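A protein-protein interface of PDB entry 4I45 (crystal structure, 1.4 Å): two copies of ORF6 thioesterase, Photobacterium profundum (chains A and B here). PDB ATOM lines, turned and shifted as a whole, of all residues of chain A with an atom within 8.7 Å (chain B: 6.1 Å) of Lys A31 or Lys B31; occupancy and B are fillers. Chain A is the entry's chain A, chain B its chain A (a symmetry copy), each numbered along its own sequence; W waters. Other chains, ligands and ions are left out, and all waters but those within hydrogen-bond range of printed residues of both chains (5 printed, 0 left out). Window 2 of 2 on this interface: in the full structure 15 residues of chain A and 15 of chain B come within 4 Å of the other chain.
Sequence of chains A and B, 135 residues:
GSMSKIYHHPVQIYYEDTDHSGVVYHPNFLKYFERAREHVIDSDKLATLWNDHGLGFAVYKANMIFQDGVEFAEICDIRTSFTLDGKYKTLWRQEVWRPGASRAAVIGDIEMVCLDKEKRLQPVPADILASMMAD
Among the printed residues, pairs that only touch across the chains: Lys A31 with Tyr B25, Tyr A25 with Lys B31, Lys A31 with Lys B31, Tyr A25 with Glu B34, Glu A34 with Tyr B25, Lys A31 with Pro B27, Pro A27 with Lys B31, Pro A27 with Leu B30 and Leu A30 with Pro B27.
N of Tyr A25 is in hydrogen-bond range of O of Asp A17.
The backbone carbonyl oxygen of Tyr A25 lies close to the side-chain amide nitrogen of Asn A28 (3.5 Å).
OE2 of Glu A38 lies close to OE1 of Glu A34 (2.5 Å).
O of Tyr B25 sits close to ND2 of Asn B28.
Tyr A25 touches Lys B31, and with the chains exchanged Lys A31 touches Tyr B25.
Pro A27 touches Leu B30, and with the chains exchanged Leu A30 touches Pro B27.
Pro A27 touches Lys B31, and with the chains exchanged Lys A31 touches Pro B27.
Lys A31 touches its own counterpart, Lys B31.
11 positions are printed for both chains.
Water W4 bridges OE1 of Glu A34 (2.6 Å) and OH of Tyr B25 (2.7 Å).
Water W5 bridges OE1 of Glu B34 (2.6 Å) and OH of Tyr A25 (2.7 Å).
Water W1 lies within hydrogen-bond range of a ring nitrogen (NE2) of His A26 (2.8 Å) and the backbone carbonyl oxygen (O) of Leu B30 (2.9 Å).
Water W2 lies within hydrogen-bond range of OD1 of Asn A28 (2.8 Å), NZ of Lys B31 (2.8 Å) and NZ of Lys A31 (2.9 Å).
Water W3 lies within hydrogen-bond range of OD1 of Asn B28, NZ of Lys A31 and NZ of Lys B31.
Glu A16 touches none of the printed residues of chain B.
Printed residues of chain B within 4 Å of Lys A31: Tyr B25 (3.5 Å), Pro B27 (3.7 Å) and Lys B31 (3.7 Å).
Of the printed residues of chain B, Glu A34 touches Tyr B25.
Of the printed residues of chain A, Leu B30 touches Pro A27 (3.996 Å).
Printed residues of chain A within 4 Å of Lys B31: Tyr A25 (3.5 Å), Pro A27 (3.7 Å) and Lys A31 (3.7 Å).
The nearest printed residue of chain A that does not touch Lys B31 is Asn A28 (4.1 Å).
The nearest printed residue of chain B that does not touch Leu A30 is Leu B30 (4.6 Å).
Among the printed residues, 9 pairs touch across the chains.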
ATOM      1  N   HIS A   9       9.620 -15.336 -41.073  1.00  0.00           N
ATOM      2  CA  HIS A   9      10.725 -15.964 -40.353  1.00  0.00           C
ATOM      3  C   HIS A   9      10.437 -17.414 -40.132  1.00  0.00           C
ATOM      4  O   HIS A   9       9.398 -17.731 -39.539  1.00  0.00           O
ATOM      5  CB  HIS A   9      10.941 -15.295 -39.006  1.00  0.00           C
ATOM      6  CG  HIS A   9      12.037 -15.927 -38.204  1.00  0.00           C
ATOM      7  ND1 HIS A   9      13.335 -15.849 -38.564  1.00  0.00           N
ATOM      8  CD2 HIS A   9      11.994 -16.693 -37.042  1.00  0.00           C
ATOM      9  CE1 HIS A   9      14.083 -16.525 -37.680  1.00  0.00           C
ATOM     10  NE2 HIS A   9      13.262 -17.034 -36.741  1.00  0.00           N
ATOM     11  N   VAL A  11      10.510 -21.137 -38.534  1.00  0.00           N
ATOM     12  CA  VAL A  11      10.840 -21.792 -37.272  1.00  0.00           C
ATOM     13  C   VAL A  11      10.649 -23.298 -37.449  1.00  0.00           C
ATOM     14  O   VAL A  11       9.601 -23.759 -37.921  1.00  0.00           O
ATOM     15  CB  VAL A  11       9.996 -21.296 -36.100  1.00  0.00           C
ATOM     16  CG1 VAL A  11      10.392 -22.013 -34.803  1.00  0.00           C
ATOM     17  CG2 VAL A  11      10.128 -19.756 -35.947  1.00  0.00           C
ATOM     18  N   GLU A  16      13.510 -29.638 -28.111  1.00  0.00           N
ATOM     19  CA  GLU A  16      13.445 -28.559 -27.102  1.00  0.00           C
ATOM     20  C   GLU A  16      12.138 -27.786 -27.069  1.00  0.00           C
ATOM     21  O   GLU A  16      11.821 -27.187 -26.055  1.00  0.00           O
ATOM     22  CB  GLU A  16      14.571 -27.548 -27.336  1.00  0.00           C
ATOM     23  CG  GLU A  16      14.390 -26.727 -28.598  1.00  0.00           C
ATOM     24  CD  GLU A  16      15.665 -26.071 -29.045  1.00  0.00           C
ATOM     25  OE1 GLU A  16      15.743 -24.825 -28.866  1.00  0.00           O
ATOM     26  OE2 GLU A  16      16.572 -26.751 -29.528  1.00  0.00           O
ATOM     27  N   ASP A  17      11.369 -27.854 -28.160  1.00  0.00           N
ATOM     28  CA  ASP A  17      10.170 -27.077 -28.348  1.00  0.00           C
ATOM     29  C   ASP A  17       8.849 -27.718 -27.899  1.00  0.00           C
ATOM     30  O   ASP A  17       7.870 -27.032 -27.666  1.00  0.00           O
ATOM     31  CB  ASP A  17      10.074 -26.700 -29.807  1.00  0.00           C
ATOM     32  CG  ASP A  17      11.243 -25.840 -30.263  1.00  0.00           C
ATOM     33  OD1 ASP A  17      11.370 -24.744 -29.658  1.00  0.00           O
ATOM     34  OD2 ASP A  17      12.002 -26.194 -31.180  1.00  0.00           O
ATOM     35  N   TYR A  25       5.142 -26.568 -26.620  1.00  0.00           N
ATOM     36  CA  TYR A  25       4.805 -26.067 -25.297  1.00  0.00           C
ATOM     37  C   TYR A  25       4.471 -24.566 -25.456  1.00  0.00           C
ATOM     38  O   TYR A  25       5.300 -23.789 -25.985  1.00  0.00           O
ATOM     39  CB  TYR A  25       6.022 -26.266 -24.391  1.00  0.00           C
ATOM     40  CG  TYR A  25       5.946 -25.653 -23.035  1.00  0.00           C
ATOM     41  CD1 TYR A  25       4.933 -25.981 -22.160  1.00  0.00           C
ATOM     42  CD2 TYR A  25       6.923 -24.756 -22.610  1.00  0.00           C
ATOM     43  CE1 TYR A  25       4.857 -25.414 -20.898  1.00  0.00           C
ATOM     44  CE2 TYR A  25       6.859 -24.180 -21.383  1.00  0.00           C
ATOM     45  CZ  TYR A  25       5.829 -24.486 -20.505  1.00  0.00           C
ATOM     46  OH  TYR A  25       5.764 -23.888 -19.267  1.00  0.00           O
ATOM     47  N   HIS A  26       3.277 -24.147 -25.064  1.00  0.00           N
ATOM     48  CA  HIS A  26       2.721 -22.864 -25.502  1.00  0.00           C
ATOM     49  C   HIS A  26       3.546 -21.615 -25.186  1.00  0.00           C
ATOM     50  O   HIS A  26       3.546 -20.743 -26.014  1.00  0.00           O
ATOM     51  CB  HIS A  26       1.248 -22.701 -25.099  1.00  0.00           C
ATOM     52  CG  HIS A  26       1.033 -22.510 -23.638  1.00  0.00           C
ATOM     53  ND1 HIS A  26       0.913 -23.529 -22.760  1.00  0.00           N
ATOM     54  CD2 HIS A  26       0.931 -21.334 -22.888  1.00  0.00           C
ATOM     55  CE1 HIS A  26       0.763 -23.038 -21.520  1.00  0.00           C
ATOM     56  NE2 HIS A  26       0.769 -21.688 -21.599  1.00  0.00           N
ATOM     57  N   PRO A  27       4.238 -21.596 -24.050  1.00  0.00           N
ATOM     58  CA  PRO A  27       5.048 -20.386 -23.831  1.00  0.00           C
ATOM     59  C   PRO A  27       6.091 -20.182 -24.902  1.00  0.00           C
ATOM     60  O   PRO A  27       6.606 -19.047 -25.051  1.00  0.00           O
ATOM     61  CB  PRO A  27       5.696 -20.669 -22.470  1.00  0.00           C
ATOM     62  CG  PRO A  27       4.654 -21.451 -21.743  1.00  0.00           C
ATOM     63  CD  PRO A  27       4.207 -22.411 -22.831  1.00  0.00           C
ATOM     64  N   ASN A  28       6.518 -21.209 -25.588  1.00  0.00           N
ATOM     65  CA  ASN A  28       7.519 -21.069 -26.629  1.00  0.00           C
ATOM     66  C   ASN A  28       7.132 -20.190 -27.791  1.00  0.00           C
ATOM     67  O   ASN A  28       8.014 -19.609 -28.471  1.00  0.00           O
ATOM     68  CB  ASN A  28       8.007 -22.433 -27.156  1.00  0.00           C
ATOM     69  CG  ASN A  28       8.707 -23.230 -26.108  1.00  0.00           C
ATOM     70  OD1 ASN A  28       9.248 -22.670 -25.125  1.00  0.00           O
ATOM     71  ND2 ASN A  28       8.676 -24.561 -26.251  1.00  0.00           N
ATOM     72  N   PHE A  29       5.847 -20.054 -28.076  1.00  0.00           N
ATOM     73  CA  PHE A  29       5.464 -19.245 -29.198  1.00  0.00           C
ATOM     74  C   PHE A  29       5.898 -17.768 -29.034  1.00  0.00           C
ATOM     75  O   PHE A  29       6.232 -17.108 -30.016  1.00  0.00           O
ATOM     76  CB  PHE A  29       3.979 -19.342 -29.501  1.00  0.00           C
ATOM     77  CG  PHE A  29       3.574 -20.711 -30.014  1.00  0.00           C
ATOM     78  CD1 PHE A  29       3.932 -21.054 -31.272  1.00  0.00           C
ATOM     79  CD2 PHE A  29       2.945 -21.613 -29.201  1.00  0.00           C
ATOM     80  CE1 PHE A  29       3.573 -22.287 -31.797  1.00  0.00           C
ATOM     81  CE2 PHE A  29       2.605 -22.882 -29.690  1.00  0.00           C
ATOM     82  CZ  PHE A  29       2.931 -23.208 -30.992  1.00  0.00           C
ATOM     83  N   LEU A  30       5.822 -17.272 -27.814  1.00  0.00           N
ATOM     84  CA  LEU A  30       6.297 -15.900 -27.578  1.00  0.00           C
ATOM     85  C   LEU A  30       7.791 -15.758 -27.873  1.00  0.00           C
ATOM     86  O   LEU A  30       8.214 -14.664 -28.279  1.00  0.00           O
ATOM     87  CB  LEU A  30       5.942 -15.436 -26.170  1.00  0.00           C
ATOM     88  CG  LEU A  30       4.774 -14.462 -25.998  1.00  0.00           C
ATOM     89  CD1 LEU A  30       4.697 -14.020 -24.539  1.00  0.00           C
ATOM     90  CD2 LEU A  30       4.796 -13.197 -26.925  1.00  0.00           C
ATOM     91  N   LYS A  31       8.586 -16.783 -27.589  1.00  0.00           N
ATOM     92  CA  LYS A  31       9.986 -16.805 -27.983  1.00  0.00           C
ATOM     93  C   LYS A  31      10.141 -16.693 -29.490  1.00  0.00           C
ATOM     94  O   LYS A  31      10.967 -15.941 -29.970  1.00  0.00           O
ATOM     95  CB  LYS A  31      10.756 -18.024 -27.454  1.00  0.00           C
ATOM     96  CG  LYS A  31      10.614 -18.332 -25.980  1.00  0.00           C
ATOM     97  CD  LYS A  31      11.660 -19.374 -25.565  1.00  0.00           C
ATOM     98  CE  LYS A  31      11.803 -19.551 -24.055  1.00  0.00           C
ATOM     99  NZ  LYS A  31      12.948 -20.471 -23.744  1.00  0.00           N
ATOM    100  N   TYR A  32       9.377 -17.483 -30.248  1.00  0.00           N
ATOM    101  CA  TYR A  32       9.501 -17.446 -31.686  1.00  0.00           C
ATOM    102  C   TYR A  32       9.133 -16.048 -32.193  1.00  0.00           C
ATOM    103  O   TYR A  32       9.766 -15.543 -33.141  1.00  0.00           O
ATOM    104  CB  TYR A  32       8.611 -18.530 -32.375  1.00  0.00           C
ATOM    105  CG  TYR A  32       8.736 -19.928 -31.799  1.00  0.00           C
ATOM    106  CD1 TYR A  32       9.939 -20.409 -31.299  1.00  0.00           C
ATOM    107  CD2 TYR A  32       7.631 -20.787 -31.820  1.00  0.00           C
ATOM    108  CE1 TYR A  32      10.038 -21.670 -30.744  1.00  0.00           C
ATOM    109  CE2 TYR A  32       7.724 -22.039 -31.283  1.00  0.00           C
ATOM    110  CZ  TYR A  32       8.922 -22.495 -30.768  1.00  0.00           C
ATOM    111  OH  TYR A  32       9.009 -23.752 -30.216  1.00  0.00           O
ATOM    112  N   PHE A  33       8.082 -15.471 -31.627  1.00  0.00           N
ATOM    113  CA  PHE A  33       7.721 -14.105 -31.953  1.00  0.00           C
ATOM    114  C   PHE A  33       8.853 -13.106 -31.655  1.00  0.00           C
ATOM    115  O   PHE A  33       9.136 -12.245 -32.485  1.00  0.00           O
ATOM    116  CB  PHE A  33       6.438 -13.705 -31.260  1.00  0.00           C
ATOM    117  CG  PHE A  33       5.181 -14.407 -31.786  1.00  0.00           C
ATOM    118  CD1 PHE A  33       5.158 -15.069 -33.020  1.00  0.00           C
ATOM    119  CD2 PHE A  33       4.014 -14.285 -31.098  1.00  0.00           C
ATOM    120  CE1 PHE A  33       3.972 -15.675 -33.482  1.00  0.00           C
ATOM    121  CE2 PHE A  33       2.833 -14.897 -31.561  1.00  0.00           C
ATOM    122  CZ  PHE A  33       2.827 -15.553 -32.763  1.00  0.00           C
ATOM    123  N   GLU A  34       9.515 -13.295 -30.533  1.00  0.00           N
ATOM    124  CA  GLU A  34      10.644 -12.407 -30.203  1.00  0.00           C
ATOM    125  C   GLU A  34      11.736 -12.573 -31.268  1.00  0.00           C
ATOM    126  O   GLU A  34      12.264 -11.577 -31.799  1.00  0.00           O
ATOM    127  CB  GLU A  34      11.123 -12.735 -28.807  1.00  0.00           C
ATOM    128  CG  GLU A  34      11.965 -11.627 -28.172  1.00  0.00           C
ATOM    129  CD  GLU A  34      13.364 -11.517 -28.729  1.00  0.00           C
ATOM    130  OE1 GLU A  34      13.959 -12.490 -29.210  1.00  0.00           O
ATOM    131  OE2 GLU A  34      13.883 -10.403 -28.661  1.00  0.00           O
ATOM    132  N   ARG A  35      12.114 -13.804 -31.593  1.00  0.00           N
ATOM    133  CA  ARG A  35      13.070 -14.042 -32.675  1.00  0.00           C
ATOM    134  C   ARG A  35      12.722 -13.337 -33.950  1.00  0.00           C
ATOM    135  O   ARG A  35      13.585 -12.698 -34.578  1.00  0.00           O
ATOM    136  CB  ARG A  35      13.169 -15.506 -33.053  1.00  0.00           C
ATOM    137  CG  ARG A  35      13.775 -16.336 -32.065  1.00  0.00           C
ATOM    138  CD  ARG A  35      13.747 -17.806 -32.576  1.00  0.00           C
ATOM    139  NE  ARG A  35      13.803 -18.727 -31.468  1.00  0.00           N
ATOM    140  CZ  ARG A  35      13.616 -20.042 -31.575  1.00  0.00           C
ATOM    141  NH1 ARG A  35      13.359 -20.598 -32.753  1.00  0.00           N
ATOM    142  NH2 ARG A  35      13.672 -20.747 -30.473  1.00  0.00           N
ATOM    143  N   ALA A  36      11.473 -13.492 -34.380  1.00  0.00           N
ATOM    144  CA  ALA A  36      11.033 -12.905 -35.624  1.00  0.00           C
ATOM    145  C   ALA A  36      11.184 -11.378 -35.578  1.00  0.00           C
ATOM    146  O   ALA A  36      11.535 -10.769 -36.603  1.00  0.00           O
ATOM    147  CB  ALA A  36       9.580 -13.297 -35.951  1.00  0.00           C
ATOM    148  N   ARG A  37      10.869 -10.789 -34.424  1.00  0.00           N
ATOM    149  CA  ARG A  37      11.050  -9.328 -34.267  1.00  0.00           C
ATOM    150  C   ARG A  37      12.522  -8.962 -34.379  1.00  0.00           C
ATOM    151  O   ARG A  37      12.823  -7.850 -34.882  1.00  0.00           O
ATOM    152  CB  ARG A  37      10.451  -8.782 -32.964  1.00  0.00           C
ATOM    153  CG  ARG A  37       8.894  -8.855 -32.977  1.00  0.00           C
ATOM    154  CD  ARG A  37       8.254  -8.053 -31.839  1.00  0.00           C
ATOM    155  NE  ARG A  37       8.842  -8.308 -30.540  1.00  0.00           N
ATOM    156  CZ  ARG A  37       8.476  -9.283 -29.723  1.00  0.00           C
ATOM    157  NH1 ARG A  37       7.482 -10.109 -30.079  1.00  0.00           N
ATOM    158  NH2 ARG A  37       9.035  -9.482 -28.567  1.00  0.00           N
ATOM    159  N   GLU A  38      13.430  -9.814 -33.893  1.00  0.00           N
ATOM    160  CA  GLU A  38      14.876  -9.545 -34.038  1.00  0.00           C
ATOM    161  C   GLU A  38      15.323  -9.536 -35.483  1.00  0.00           C
ATOM    162  O   GLU A  38      16.374  -8.972 -35.806  1.00  0.00           O
ATOM    163  CB  GLU A  38      15.779 -10.454 -33.218  1.00  0.00           C
ATOM    164  CG  GLU A  38      15.527 -10.476 -31.700  1.00  0.00           C
ATOM    165  CD  GLU A  38      16.613 -11.194 -30.907  1.00  0.00           C
ATOM    166  OE1 GLU A  38      17.793 -11.123 -31.303  1.00  0.00           O
ATOM    167  OE2 GLU A  38      16.302 -11.794 -29.853  1.00  0.00           O
ATOM    168  N   MET A  64      -2.140 -13.466 -26.795  1.00  0.00           N
ATOM    169  CA  MET A  64      -1.935 -14.701 -27.556  1.00  0.00           C
ATOM    170  C   MET A  64      -3.254 -15.487 -27.721  1.00  0.00           C
ATOM    171  O   MET A  64      -4.021 -15.592 -26.748  1.00  0.00           O
ATOM    172  CB  MET A  64      -0.933 -15.601 -26.815  1.00  0.00           C
ATOM    173  CG  MET A  64       0.477 -14.950 -26.591  1.00  0.00           C
ATOM    174  SD  MET A  64       1.417 -14.711 -28.127  1.00  0.00           S
ATOM    175  CE  MET A  64       2.007 -16.369 -28.498  1.00  0.00           C
ATOM    176  N   ILE A  78       6.602 -17.719 -39.413  1.00  0.00           N
ATOM    177  CA  ILE A  78       6.147 -16.636 -38.558  1.00  0.00           C
ATOM    178  C   ILE A  78       5.989 -15.395 -39.445  1.00  0.00           C
ATOM    179  O   ILE A  78       6.960 -14.915 -40.052  1.00  0.00           O
ATOM    180  CB  ILE A  78       7.129 -16.283 -37.424  1.00  0.00           C
ATOM    181  CG1 ILE A  78       7.525 -17.525 -36.607  1.00  0.00           C
ATOM    182  CG2 ILE A  78       6.510 -15.225 -36.537  1.00  0.00           C
ATOM    183  CD1 ILE A  78       6.454 -18.085 -35.779  1.00  0.00           C
ATOM    184  N   GLN A  94       1.692 -10.787 -35.025  1.00  0.00           N
ATOM    185  CA  GLN A  94       2.538 -11.912 -35.349  1.00  0.00           C
ATOM    186  C   GLN A  94       1.724 -13.197 -35.383  1.00  0.00           C
ATOM    187  O   GLN A  94       0.896 -13.415 -34.515  1.00  0.00           O
ATOM    188  CB  GLN A  94       3.714 -12.006 -34.385  1.00  0.00           C
ATOM    189  CG  GLN A  94       4.545 -10.719 -34.391  1.00  0.00           C
ATOM    190  CD  GLN A  94       5.834 -10.887 -33.622  1.00  0.00           C
ATOM    191  OE1 GLN A  94       5.879 -10.563 -32.412  1.00  0.00           O
ATOM    192  NE2 GLN A  94       6.869 -11.424 -34.275  1.00  0.00           N
ATOM    193  N   TYR B  25      13.563 -12.705 -18.969  1.00  0.00           N
ATOM    194  CA  TYR B  25      13.206 -12.736 -20.378  1.00  0.00           C
ATOM    195  C   TYR B  25      11.681 -12.981 -20.449  1.00  0.00           C
ATOM    196  O   TYR B  25      11.175 -13.976 -19.880  1.00  0.00           O
ATOM    197  CB  TYR B  25      13.976 -13.882 -21.037  1.00  0.00           C
ATOM    198  CG  TYR B  25      13.615 -14.199 -22.447  1.00  0.00           C
ATOM    199  CD1 TYR B  25      13.701 -13.244 -23.437  1.00  0.00           C
ATOM    200  CD2 TYR B  25      13.214 -15.484 -22.801  1.00  0.00           C
ATOM    201  CE1 TYR B  25      13.366 -13.533 -24.750  1.00  0.00           C
ATOM    202  CE2 TYR B  25      12.868 -15.784 -24.078  1.00  0.00           C
ATOM    203  CZ  TYR B  25      12.928 -14.823 -25.076  1.00  0.00           C
ATOM    204  OH  TYR B  25      12.565 -15.131 -26.368  1.00  0.00           O
ATOM    205  N   PRO B  27       9.106 -14.054 -22.203  1.00  0.00           N
ATOM    206  CA  PRO B  27       8.323 -15.282 -22.419  1.00  0.00           C
ATOM    207  C   PRO B  27       8.329 -16.195 -21.218  1.00  0.00           C
ATOM    208  O   PRO B  27       7.447 -17.081 -21.115  1.00  0.00           O
ATOM    209  CB  PRO B  27       9.045 -15.924 -23.610  1.00  0.00           C
ATOM    210  CG  PRO B  27       9.512 -14.754 -24.409  1.00  0.00           C
ATOM    211  CD  PRO B  27      10.049 -13.855 -23.309  1.00  0.00           C
ATOM    212  N   ASN B  28       9.309 -16.119 -20.358  1.00  0.00           N
ATOM    213  CA  ASN B  28       9.364 -16.973 -19.186  1.00  0.00           C
ATOM    214  C   ASN B  28       8.222 -16.818 -18.214  1.00  0.00           C
ATOM    215  O   ASN B  28       7.891 -17.770 -17.464  1.00  0.00           O
ATOM    216  CB  ASN B  28      10.703 -16.843 -18.432  1.00  0.00           C
ATOM    217  CG  ASN B  28      11.862 -17.303 -19.249  1.00  0.00           C
ATOM    218  OD1 ASN B  28      11.708 -18.124 -20.184  1.00  0.00           O
ATOM    219  ND2 ASN B  28      13.049 -16.753 -18.963  1.00  0.00           N
ATOM    220  N   PHE B  29       7.589 -15.658 -18.166  1.00  0.00           N
ATOM    221  CA  PHE B  29       6.519 -15.485 -17.224  1.00  0.00           C
ATOM    222  C   PHE B  29       5.346 -16.463 -17.481  1.00  0.00           C
ATOM    223  O   PHE B  29       4.695 -16.907 -16.537  1.00  0.00           O
ATOM    224  CB  PHE B  29       6.025 -14.050 -17.167  1.00  0.00           C
ATOM    225  CG  PHE B  29       7.051 -13.101 -16.577  1.00  0.00           C
ATOM    226  CD1 PHE B  29       7.281 -13.155 -15.246  1.00  0.00           C
ATOM    227  CD2 PHE B  29       7.790 -12.273 -17.377  1.00  0.00           C
ATOM    228  CE1 PHE B  29       8.196 -12.298 -14.652  1.00  0.00           C
ATOM    229  CE2 PHE B  29       8.752 -11.424 -16.811  1.00  0.00           C
ATOM    230  CZ  PHE B  29       8.948 -11.451 -15.443  1.00  0.00           C
ATOM    231  N   LEU B  30       5.069 -16.720 -18.744  1.00  0.00           N
ATOM    232  CA  LEU B  30       4.020 -17.703 -19.051  1.00  0.00           C
ATOM    233  C   LEU B  30       4.375 -19.096 -18.527  1.00  0.00           C
ATOM    234  O   LEU B  30       3.454 -19.853 -18.183  1.00  0.00           O
ATOM    235  CB  LEU B  30       3.704 -17.714 -20.543  1.00  0.00           C
ATOM    236  CG  LEU B  30       2.419 -17.030 -21.019  1.00  0.00           C
ATOM    237  CD1 LEU B  30       2.233 -17.293 -22.511  1.00  0.00           C
ATOM    238  CD2 LEU B  30       1.110 -17.424 -20.252  1.00  0.00           C
ATOM    239  N   LYS B  31       5.650 -19.469 -18.554  1.00  0.00           N
ATOM    240  CA  LYS B  31       6.105 -20.701 -17.929  1.00  0.00           C
ATOM    241  C   LYS B  31       5.803 -20.714 -16.441  1.00  0.00           C
ATOM    242  O   LYS B  31       5.328 -21.703 -15.917  1.00  0.00           O
ATOM    243  CB  LYS B  31       7.590 -21.005 -18.179  1.00  0.00           C
ATOM    244  CG  LYS B  31       8.070 -20.926 -19.610  1.00  0.00           C
ATOM    245  CD  LYS B  31       9.471 -21.539 -19.722  1.00  0.00           C
ATOM    246  CE  LYS B  31       9.940 -21.775 -21.156  1.00  0.00           C
ATOM    247  NZ  LYS B  31      11.247 -22.513 -21.163  1.00  0.00           N
ATOM    248  N   TYR B  32       6.127 -19.626 -15.738  1.00  0.00           N
ATOM    249  CA  TYR B  32       5.896 -19.591 -14.313  1.00  0.00           C
ATOM    250  C   TYR B  32       4.394 -19.726 -14.037  1.00  0.00           C
ATOM    251  O   TYR B  32       3.997 -20.390 -13.060  1.00  0.00           O
ATOM    252  CB  TYR B  32       6.456 -18.283 -13.665  1.00  0.00           C
ATOM    253  CG  TYR B  32       7.881 -17.933 -14.049  1.00  0.00           C
ATOM    254  CD1 TYR B  32       8.838 -18.913 -14.280  1.00  0.00           C
ATOM    255  CD2 TYR B  32       8.270 -16.590 -14.116  1.00  0.00           C
ATOM    256  CE1 TYR B  32      10.125 -18.588 -14.663  1.00  0.00           C
ATOM    257  CE2 TYR B  32       9.544 -16.262 -14.484  1.00  0.00           C
ATOM    258  CZ  TYR B  32      10.478 -17.248 -14.734  1.00  0.00           C
ATOM    259  OH  TYR B  32      11.757 -16.914 -15.116  1.00  0.00           O
ATOM    260  N   PHE B  33       3.583 -19.043 -14.835  1.00  0.00           N
ATOM    261  CA  PHE B  33       2.144 -19.193 -14.733  1.00  0.00           C
ATOM    262  C   PHE B  33       1.683 -20.646 -14.947  1.00  0.00           C
ATOM    263  O   PHE B  33       0.854 -21.137 -14.185  1.00  0.00           O
ATOM    264  CB  PHE B  33       1.434 -18.246 -15.673  1.00  0.00           C
ATOM    265  CG  PHE B  33       1.539 -16.765 -15.290  1.00  0.00           C
ATOM    266  CD1 PHE B  33       1.931 -16.353 -14.010  1.00  0.00           C
ATOM    267  CD2 PHE B  33       1.125 -15.819 -16.174  1.00  0.00           C
ATOM    268  CE1 PHE B  33       1.985 -14.981 -13.688  1.00  0.00           C
ATOM    269  CE2 PHE B  33       1.186 -14.449 -15.850  1.00  0.00           C
ATOM    270  CZ  PHE B  33       1.583 -14.058 -14.599  1.00  0.00           C
ATOM    271  N   GLU B  34       2.283 -21.310 -15.913  1.00  0.00           N
ATOM    272  CA  GLU B  34       1.928 -22.721 -16.146  1.00  0.00           C
ATOM    273  C   GLU B  34       2.293 -23.539 -14.900  1.00  0.00           C
ATOM    274  O   GLU B  34       1.478 -24.341 -14.405  1.00  0.00           O
ATOM    275  CB  GLU B  34       2.637 -23.195 -17.395  1.00  0.00           C
ATOM    276  CG  GLU B  34       2.028 -24.461 -18.001  1.00  0.00           C
ATOM    277  CD  GLU B  34       2.334 -25.724 -17.233  1.00  0.00           C
ATOM    278  OE1 GLU B  34       3.360 -25.846 -16.550  1.00  0.00           O
ATOM    279  OE2 GLU B  34       1.509 -26.630 -17.338  1.00  0.00           O
ATOM    280  N   ARG B  35       3.504 -23.382 -14.378  1.00  0.00           N
ATOM    281  CA  ARG B  35       3.882 -24.047 -13.131  1.00  0.00           C
ATOM    282  C   ARG B  35       2.895 -23.849 -12.022  1.00  0.00           C
ATOM    283  O   ARG B  35       2.512 -24.812 -11.334  1.00  0.00           O
ATOM    284  CB  ARG B  35       5.198 -23.539 -12.577  1.00  0.00           C
ATOM    285  CG  ARG B  35       6.344 -23.893 -13.348  1.00  0.00           C
ATOM    286  CD  ARG B  35       7.598 -23.251 -12.684  1.00  0.00           C
ATOM    287  NE  ARG B  35       8.650 -23.079 -13.655  1.00  0.00           N
ATOM    288  CZ  ARG B  35       9.773 -22.397 -13.432  1.00  0.00           C
ATOM    289  NH1 ARG B  35       9.992 -21.816 -12.259  1.00  0.00           N
ATOM    290  NH2 ARG B  35      10.626 -22.306 -14.421  1.00  0.00           N
ATOM    291  N   ALA B  36       2.517 -22.595 -11.794  1.00  0.00           N
ATOM    292  CA  ALA B  36       1.611 -22.271 -10.717  1.00  0.00           C
ATOM    293  C   ALA B  36       0.271 -22.994 -10.910  1.00  0.00           C
ATOM    294  O   ALA B  36      -0.336 -23.431  -9.917  1.00  0.00           O
ATOM    295  CB  ALA B  36       1.395 -20.751 -10.597  1.00  0.00           C
HETATM  296  O   HOH W   1       0.828 -20.497 -19.115  1.00  0.00           O
HETATM  297  O   HOH W   2      11.708 -23.083 -23.911  1.00  0.00           O
HETATM  298  O   HOH W   3      13.173 -20.364 -20.911  1.00  0.00           O
HETATM  299  O   HOH W   4      14.562 -14.827 -28.167  1.00  0.00           O
HETATM  300  O   HOH W   5       5.898 -25.632 -17.203  1.00  0.00           O
